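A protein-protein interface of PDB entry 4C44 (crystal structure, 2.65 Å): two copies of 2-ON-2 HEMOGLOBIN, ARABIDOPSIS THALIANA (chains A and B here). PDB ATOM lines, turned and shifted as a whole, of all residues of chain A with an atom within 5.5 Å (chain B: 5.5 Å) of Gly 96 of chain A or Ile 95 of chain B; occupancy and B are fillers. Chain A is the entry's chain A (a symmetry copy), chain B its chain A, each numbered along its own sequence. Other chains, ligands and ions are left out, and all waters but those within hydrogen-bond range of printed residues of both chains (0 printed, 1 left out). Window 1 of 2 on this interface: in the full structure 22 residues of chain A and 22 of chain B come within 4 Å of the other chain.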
ATOM      1  N   ALA A  93      23.410 -19.149 -29.419  1.00  0.00           N
ATOM      2  CA  ALA A  93      22.929 -17.812 -28.991  1.00  0.00           C
ATOM      3  C   ALA A  93      21.740 -17.929 -28.058  1.00  0.00           C
ATOM      4  O   ALA A  93      20.643 -17.443 -28.363  1.00  0.00           O
ATOM      5  CB  ALA A  93      22.585 -16.958 -30.191  1.00  0.00           C
ATOM      6  N   LEU A  94      21.956 -18.589 -26.917  1.00  0.00           N
ATOM      7  CA  LEU A  94      20.840 -18.974 -26.061  1.00  0.00           C
ATOM      8  C   LEU A  94      20.055 -17.790 -25.546  1.00  0.00           C
ATOM      9  O   LEU A  94      18.822 -17.833 -25.493  1.00  0.00           O
ATOM     10  CB  LEU A  94      21.299 -19.860 -24.906  1.00  0.00           C
ATOM     11  CG  LEU A  94      21.920 -21.203 -25.297  1.00  0.00           C
ATOM     12  CD1 LEU A  94      22.262 -21.972 -24.037  1.00  0.00           C
ATOM     13  CD2 LEU A  94      21.009 -22.020 -26.203  1.00  0.00           C
ATOM     14  N   ILE A  95      20.745 -16.717 -25.182  1.00  0.00           N
ATOM     15  CA  ILE A  95      20.014 -15.594 -24.644  1.00  0.00           C
ATOM     16  C   ILE A  95      19.163 -15.006 -25.765  1.00  0.00           C
ATOM     17  O   ILE A  95      17.938 -14.869 -25.616  1.00  0.00           O
ATOM     18  CB  ILE A  95      20.926 -14.555 -23.983  1.00  0.00           C
ATOM     19  CG1 ILE A  95      21.428 -15.097 -22.638  1.00  0.00           C
ATOM     20  CG2 ILE A  95      20.160 -13.265 -23.770  1.00  0.00           C
ATOM     21  CD1 ILE A  95      22.427 -14.216 -21.914  1.00  0.00           C
ATOM     22  N   GLY A  96      19.808 -14.718 -26.899  1.00  0.00           N
ATOM     23  CA  GLY A  96      19.111 -14.203 -28.073  1.00  0.00           C
ATOM     24  C   GLY A  96      17.898 -15.034 -28.461  1.00  0.00           C
ATOM     25  O   GLY A  96      16.803 -14.504 -28.634  1.00  0.00           O
ATOM     26  N   ARG A  97      18.069 -16.347 -28.559  1.00  0.00           N
ATOM     27  CA  ARG A  97      16.954 -17.192 -28.996  1.00  0.00           C
ATOM     28  C   ARG A  97      15.846 -17.368 -27.945  1.00  0.00           C
ATOM     29  O   ARG A  97      14.760 -17.855 -28.277  1.00  0.00           O
ATOM     30  CB  ARG A  97      17.456 -18.533 -29.525  1.00  0.00           C
ATOM     31  CG  ARG A  97      18.759 -18.402 -30.296  1.00  0.00           C
ATOM     32  CD  ARG A  97      19.193 -19.687 -30.987  1.00  0.00           C
ATOM     33  NE  ARG A  97      18.669 -19.636 -32.335  1.00  0.00           N
ATOM     34  CZ  ARG A  97      19.375 -19.511 -33.449  1.00  0.00           C
ATOM     35  NH1 ARG A  97      20.693 -19.484 -33.446  1.00  0.00           N
ATOM     36  NH2 ARG A  97      18.719 -19.443 -34.587  1.00  0.00           N
ATOM     37  N   HIS A  98      16.102 -16.962 -26.696  1.00  0.00           N
ATOM     38  CA  HIS A  98      15.057 -16.995 -25.652  1.00  0.00           C
ATOM     39  C   HIS A  98      14.436 -15.623 -25.410  1.00  0.00           C
ATOM     40  O   HIS A  98      13.515 -15.501 -24.610  1.00  0.00           O
ATOM     41  CB  HIS A  98      15.571 -17.549 -24.324  1.00  0.00           C
ATOM     42  CG  HIS A  98      15.733 -19.030 -24.306  1.00  0.00           C
ATOM     43  ND1 HIS A  98      16.851 -19.661 -24.810  1.00  0.00           N
ATOM     44  CD2 HIS A  98      14.932 -20.010 -23.824  1.00  0.00           C
ATOM     45  CE1 HIS A  98      16.722 -20.969 -24.657  1.00  0.00           C
ATOM     46  NE2 HIS A  98      15.570 -21.205 -24.052  1.00  0.00           N
ATOM     47  N   ARG A  99      14.933 -14.597 -26.098  1.00  0.00           N
ATOM     48  CA  ARG A  99      14.348 -13.247 -26.013  1.00  0.00           C
ATOM     49  C   ARG A  99      12.800 -13.186 -26.087  1.00  0.00           C
ATOM     50  O   ARG A  99      12.185 -12.485 -25.282  1.00  0.00           O
ATOM     51  CB  ARG A  99      14.987 -12.325 -27.047  1.00  0.00           C
ATOM     52  CG  ARG A  99      14.645 -10.852 -26.890  1.00  0.00           C
ATOM     53  CD  ARG A  99      15.608  -9.999 -27.703  1.00  0.00           C
ATOM     54  NE  ARG A  99      16.973 -10.092 -27.168  1.00  0.00           N
ATOM     55  CZ  ARG A  99      18.087  -9.720 -27.807  1.00  0.00           C
ATOM     56  NH1 ARG A  99      18.050  -9.228 -29.046  1.00  0.00           N
ATOM     57  NH2 ARG A  99      19.257  -9.851 -27.196  1.00  0.00           N
ATOM     58  N   PRO A 100      12.164 -13.935 -27.020  1.00  0.00           N
ATOM     59  CA  PRO A 100      10.701 -13.854 -27.111  1.00  0.00           C
ATOM     60  C   PRO A 100       9.947 -14.401 -25.897  1.00  0.00           C
ATOM     61  O   PRO A 100       8.768 -14.121 -25.750  1.00  0.00           O
ATOM     62  CB  PRO A 100      10.366 -14.731 -28.334  1.00  0.00           C
ATOM     63  CG  PRO A 100      11.647 -14.925 -29.069  1.00  0.00           C
ATOM     64  CD  PRO A 100      12.710 -14.877 -28.017  1.00  0.00           C
ATOM     65  N   LEU B   4      16.955 -15.309 -36.987  1.00  0.00           N
ATOM     66  CA  LEU B   4      18.244 -14.648 -36.850  1.00  0.00           C
ATOM     67  C   LEU B   4      19.283 -15.075 -37.896  1.00  0.00           C
ATOM     68  O   LEU B   4      19.923 -14.228 -38.540  1.00  0.00           O
ATOM     69  CB  LEU B   4      18.777 -14.865 -35.432  1.00  0.00           C
ATOM     70  CG  LEU B   4      18.555 -13.801 -34.349  1.00  0.00           C
ATOM     71  CD1 LEU B   4      17.596 -12.698 -34.754  1.00  0.00           C
ATOM     72  CD2 LEU B   4      18.094 -14.473 -33.078  1.00  0.00           C
ATOM     73  N   ALA B  93      27.035 -17.148 -25.750  1.00  0.00           N
ATOM     74  CA  ALA B  93      25.856 -16.247 -25.757  1.00  0.00           C
ATOM     75  C   ALA B  93      26.166 -14.945 -26.467  1.00  0.00           C
ATOM     76  O   ALA B  93      26.099 -13.863 -25.868  1.00  0.00           O
ATOM     77  CB  ALA B  93      25.373 -15.987 -24.348  1.00  0.00           C
ATOM     78  N   LEU B  94      26.516 -15.049 -27.752  1.00  0.00           N
ATOM     79  CA  LEU B  94      27.067 -13.902 -28.465  1.00  0.00           C
ATOM     80  C   LEU B  94      26.108 -12.736 -28.539  1.00  0.00           C
ATOM     81  O   LEU B  94      26.517 -11.581 -28.382  1.00  0.00           O
ATOM     82  CB  LEU B  94      27.553 -14.290 -29.859  1.00  0.00           C
ATOM     83  CG  LEU B  94      28.689 -15.314 -29.913  1.00  0.00           C
ATOM     84  CD1 LEU B  94      29.082 -15.536 -31.359  1.00  0.00           C
ATOM     85  CD2 LEU B  94      29.891 -14.889 -29.081  1.00  0.00           C
ATOM     86  N   ILE B  95      24.830 -13.016 -28.753  1.00  0.00           N
ATOM     87  CA  ILE B  95      23.908 -11.911 -28.873  1.00  0.00           C
ATOM     88  C   ILE B  95      23.815 -11.226 -27.513  1.00  0.00           C
ATOM     89  O   ILE B  95      24.035 -10.009 -27.407  1.00  0.00           O
ATOM     90  CB  ILE B  95      22.540 -12.336 -29.419  1.00  0.00           C
ATOM     91  CG1 ILE B  95      22.658 -12.628 -30.920  1.00  0.00           C
ATOM     92  CG2 ILE B  95      21.530 -11.232 -29.182  1.00  0.00           C
ATOM     93  CD1 ILE B  95      21.400 -13.162 -31.579  1.00  0.00           C
ATOM     94  N   GLY B  96      23.548 -12.023 -26.475  1.00  0.00           N
ATOM     95  CA  GLY B  96      23.485 -11.515 -25.108  1.00  0.00           C
ATOM     96  C   GLY B  96      24.701 -10.689 -24.721  1.00  0.00           C
ATOM     97  O   GLY B  96      24.571  -9.566 -24.238  1.00  0.00           O
ATOM     98  N   ARG B  97      25.895 -11.215 -24.968  1.00  0.00           N
ATOM     99  CA  ARG B  97      27.103 -10.496 -24.555  1.00  0.00           C
ATOM    100  C   ARG B  97      27.422  -9.256 -25.406  1.00  0.00           C
ATOM    101  O   ARG B  97      28.269  -8.446 -25.014  1.00  0.00           O
ATOM    102  CB  ARG B  97      28.298 -11.441 -24.456  1.00  0.00           C
ATOM    103  CG  ARG B  97      27.913 -12.809 -23.917  1.00  0.00           C
ATOM    104  CD  ARG B  97      29.103 -13.714 -23.637  1.00  0.00           C
ATOM    105  NE  ARG B  97      29.453 -13.530 -22.245  1.00  0.00           N
ATOM    106  CZ  ARG B  97      29.316 -14.421 -21.275  1.00  0.00           C
ATOM    107  NH1 ARG B  97      28.887 -15.648 -21.504  1.00  0.00           N
ATOM    108  NH2 ARG B  97      29.653 -14.060 -20.057  1.00  0.00           N
ATOM    109  N   HIS B  98      26.745  -9.094 -26.549  1.00  0.00           N
ATOM    110  CA  HIS B  98      26.911  -7.877 -27.370  1.00  0.00           C
ATOM    111  C   HIS B  98      25.775  -6.881 -27.167  1.00  0.00           C
ATOM    112  O   HIS B  98      25.802  -5.796 -27.741  1.00  0.00           O
ATOM    113  CB  HIS B  98      27.039  -8.188 -28.861  1.00  0.00           C
ATOM    114  CG  HIS B  98      28.373  -8.723 -29.257  1.00  0.00           C
ATOM    115  ND1 HIS B  98      28.710 -10.052 -29.122  1.00  0.00           N
ATOM    116  CD2 HIS B  98      29.450  -8.114 -29.810  1.00  0.00           C
ATOM    117  CE1 HIS B  98      29.946 -10.237 -29.555  1.00  0.00           C
ATOM    118  NE2 HIS B  98      30.413  -9.078 -29.987  1.00  0.00           N
ATOM    119  N   ARG B  99      24.784  -7.240 -26.355  1.00  0.00           N
ATOM    120  CA  ARG B  99      23.685  -6.320 -26.013  1.00  0.00           C
ATOM    121  C   ARG B  99      24.114  -4.873 -25.656  1.00  0.00           C
ATOM    122  O   ARG B  99      23.505  -3.924 -26.150  1.00  0.00           O
ATOM    123  CB  ARG B  99      22.808  -6.922 -24.919  1.00  0.00           C
ATOM    124  CG  ARG B  99      21.507  -6.180 -24.659  1.00  0.00           C
ATOM    125  CD  ARG B  99      20.557  -7.051 -23.850  1.00  0.00           C
ATOM    126  NE  ARG B  99      20.132  -8.226 -24.623  1.00  0.00           N
ATOM    127  CZ  ARG B  99      19.557  -9.322 -24.120  1.00  0.00           C
ATOM    128  NH1 ARG B  99      19.325  -9.453 -22.813  1.00  0.00           N
ATOM    129  NH2 ARG B  99      19.214 -10.306 -24.941  1.00  0.00           N
ATOM    130  N   PHE B 143      24.726 -11.721 -38.093  1.00  0.00           N
ATOM    131  CA  PHE B 143      23.892 -12.390 -37.114  1.00  0.00           C
ATOM    132  C   PHE B 143      23.804 -11.473 -35.887  1.00  0.00           C
ATOM    133  O   PHE B 143      22.701 -11.215 -35.386  1.00  0.00           O
ATOM    134  CB  PHE B 143      24.541 -13.728 -36.809  1.00  0.00           C
ATOM    135  CG  PHE B 143      23.820 -14.559 -35.805  1.00  0.00           C
ATOM    136  CD1 PHE B 143      22.792 -15.415 -36.193  1.00  0.00           C
ATOM    137  CD2 PHE B 143      24.220 -14.553 -34.470  1.00  0.00           C
ATOM    138  CE1 PHE B 143      22.145 -16.211 -35.258  1.00  0.00           C
ATOM    139  CE2 PHE B 143      23.574 -15.349 -33.534  1.00  0.00           C
ATOM    140  CZ  PHE B 143      22.542 -16.179 -33.933  1.00  0.00           C
ATOM    141  N   LEU B 144      24.945 -10.927 -35.446  1.00  0.00           N
ATOM    142  CA  LEU B 144      24.942  -9.924 -34.349  1.00  0.00           C
ATOM    143  C   LEU B 144      24.152  -8.645 -34.685  1.00  0.00           C
ATOM    144  O   LEU B 144      23.360  -8.167 -33.866  1.00  0.00           O
ATOM    145  CB  LEU B 144      26.361  -9.595 -33.859  1.00  0.00           C
ATOM    146  CG  LEU B 144      27.119 -10.754 -33.205  1.00  0.00           C
ATOM    147  CD1 LEU B 144      28.533 -10.363 -32.844  1.00  0.00           C
ATOM    148  CD2 LEU B 144      26.394 -11.284 -31.975  1.00  0.00           C
ATOM    149  N   GLY B 147      20.648  -9.406 -34.337  1.00  0.00           N
ATOM    150  CA  GLY B 147      20.350  -9.536 -32.924  1.00  0.00           C
ATOM    151  C   GLY B 147      20.220  -8.179 -32.278  1.00  0.00           C
ATOM    152  O   GLY B 147      19.345  -7.963 -31.442  1.00  0.00           O
ATOM    153  N   ASN B 148      21.087  -7.256 -32.682  1.00  0.00           N
ATOM    154  CA  ASN B 148      21.031  -5.891 -32.201  1.00  0.00           C
ATOM    155  C   ASN B 148      19.727  -5.195 -32.552  1.00  0.00           C
ATOM    156  O   ASN B 148      19.318  -4.277 -31.864  1.00  0.00           O
ATOM    157  CB  ASN B 148      22.181  -5.098 -32.778  1.00  0.00           C
ATOM    158  CG  ASN B 148      22.484  -3.855 -31.975  1.00  0.00           C
ATOM    159  OD1 ASN B 148      22.237  -2.754 -32.441  1.00  0.00           O
ATOM    160  ND2 ASN B 148      23.022  -4.029 -30.756  1.00  0.00           N
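The guanidinium group (NH1) of Arg 99 of chain A lies within hydrogen-bond range of the backbone carbonyl oxygen (O) of Gly 147 of chain B, 3.0 Å away. The guanidinium group (NH2) of Arg 99 of chain A sits close to the guanidinium group (NH2) of Arg 99 of chain B, at 2.3 Å.
Ala 93 of chain A touches Phe 143 of chain B. CA of Gly 96 of chain B touches CG2 of Ile 95 of chain A (3.99 Å). NH2 of Arg 99 of chain B touches CG2 of Ile 95 of chain A, at 3.3 Å. CG2 of Ile 95 of chain B touches CA of Gly 96 of chain A, 3.99 Å away. Phe 143 of chain B touches Arg 97 of chain A. Ile 95 of chain B touches Arg 99 of chain A (CG2 to NH2, 3.3 Å).
Leu 94 of chain A touches none of the printed residues of chain B. Printed residues of chain B within 4 Å of Ile 95 of chain A: Gly 96 and Arg 99. Of the printed residues of chain B, Arg 99 of chain A touches Ile 95 (3.3 Å), Arg 99 (2.3 Å) and Gly 147 (3.0 Å). Of the printed residues of chain A, Ile 95 of chain B touches Gly 96 and Arg 99. His 98 of chain B touches none of the printed residues of chain A. Printed residues of chain A within 4 Å of Arg 99 of chain B: Ile 95 and Arg 99. Of the printed residues of chain A, Phe 143 of chain B touches Ala 93 and Arg 97. Of the printed residues of chain A, Gly 147 of chain B touches Arg 99. The nearest printed residue of chain A that does not touch Ile 95 of chain B is Ala 93 of chain A (4.2 Å).
Of the 8 printed residues of chain A, 5 touch a printed residue of chain B. Printed residues of chain A that touch a printed residue of chain B: Ala 93, Ile 95, Gly 96, Arg 97 and Arg 99. Printed residues of chain B that touch a printed residue of chain A: Ile 95, Gly 96, Arg 99, Phe 143 and Gly 147. Hydrophobic or aromatic side chains of chain B within 4 Å of the printed part of chain A: Ile 95 and Phe 143. Along chain B the printed residues that touch a printed residue of chain A span positions 95 to 147.
Ile 95 of chain A touches Gly 96 of chain B, and with the chains exchanged Gly 96 of chain A touches Ile 95 of chain B. Ile 95 of chain A touches Arg 99 of chain B, and with the chains exchanged Arg 99 of chain A touches Ile 95 of chain B. Arg 99 of chain A touches its own counterpart, Arg 99 of chain B. 7 positions are printed for both chains.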
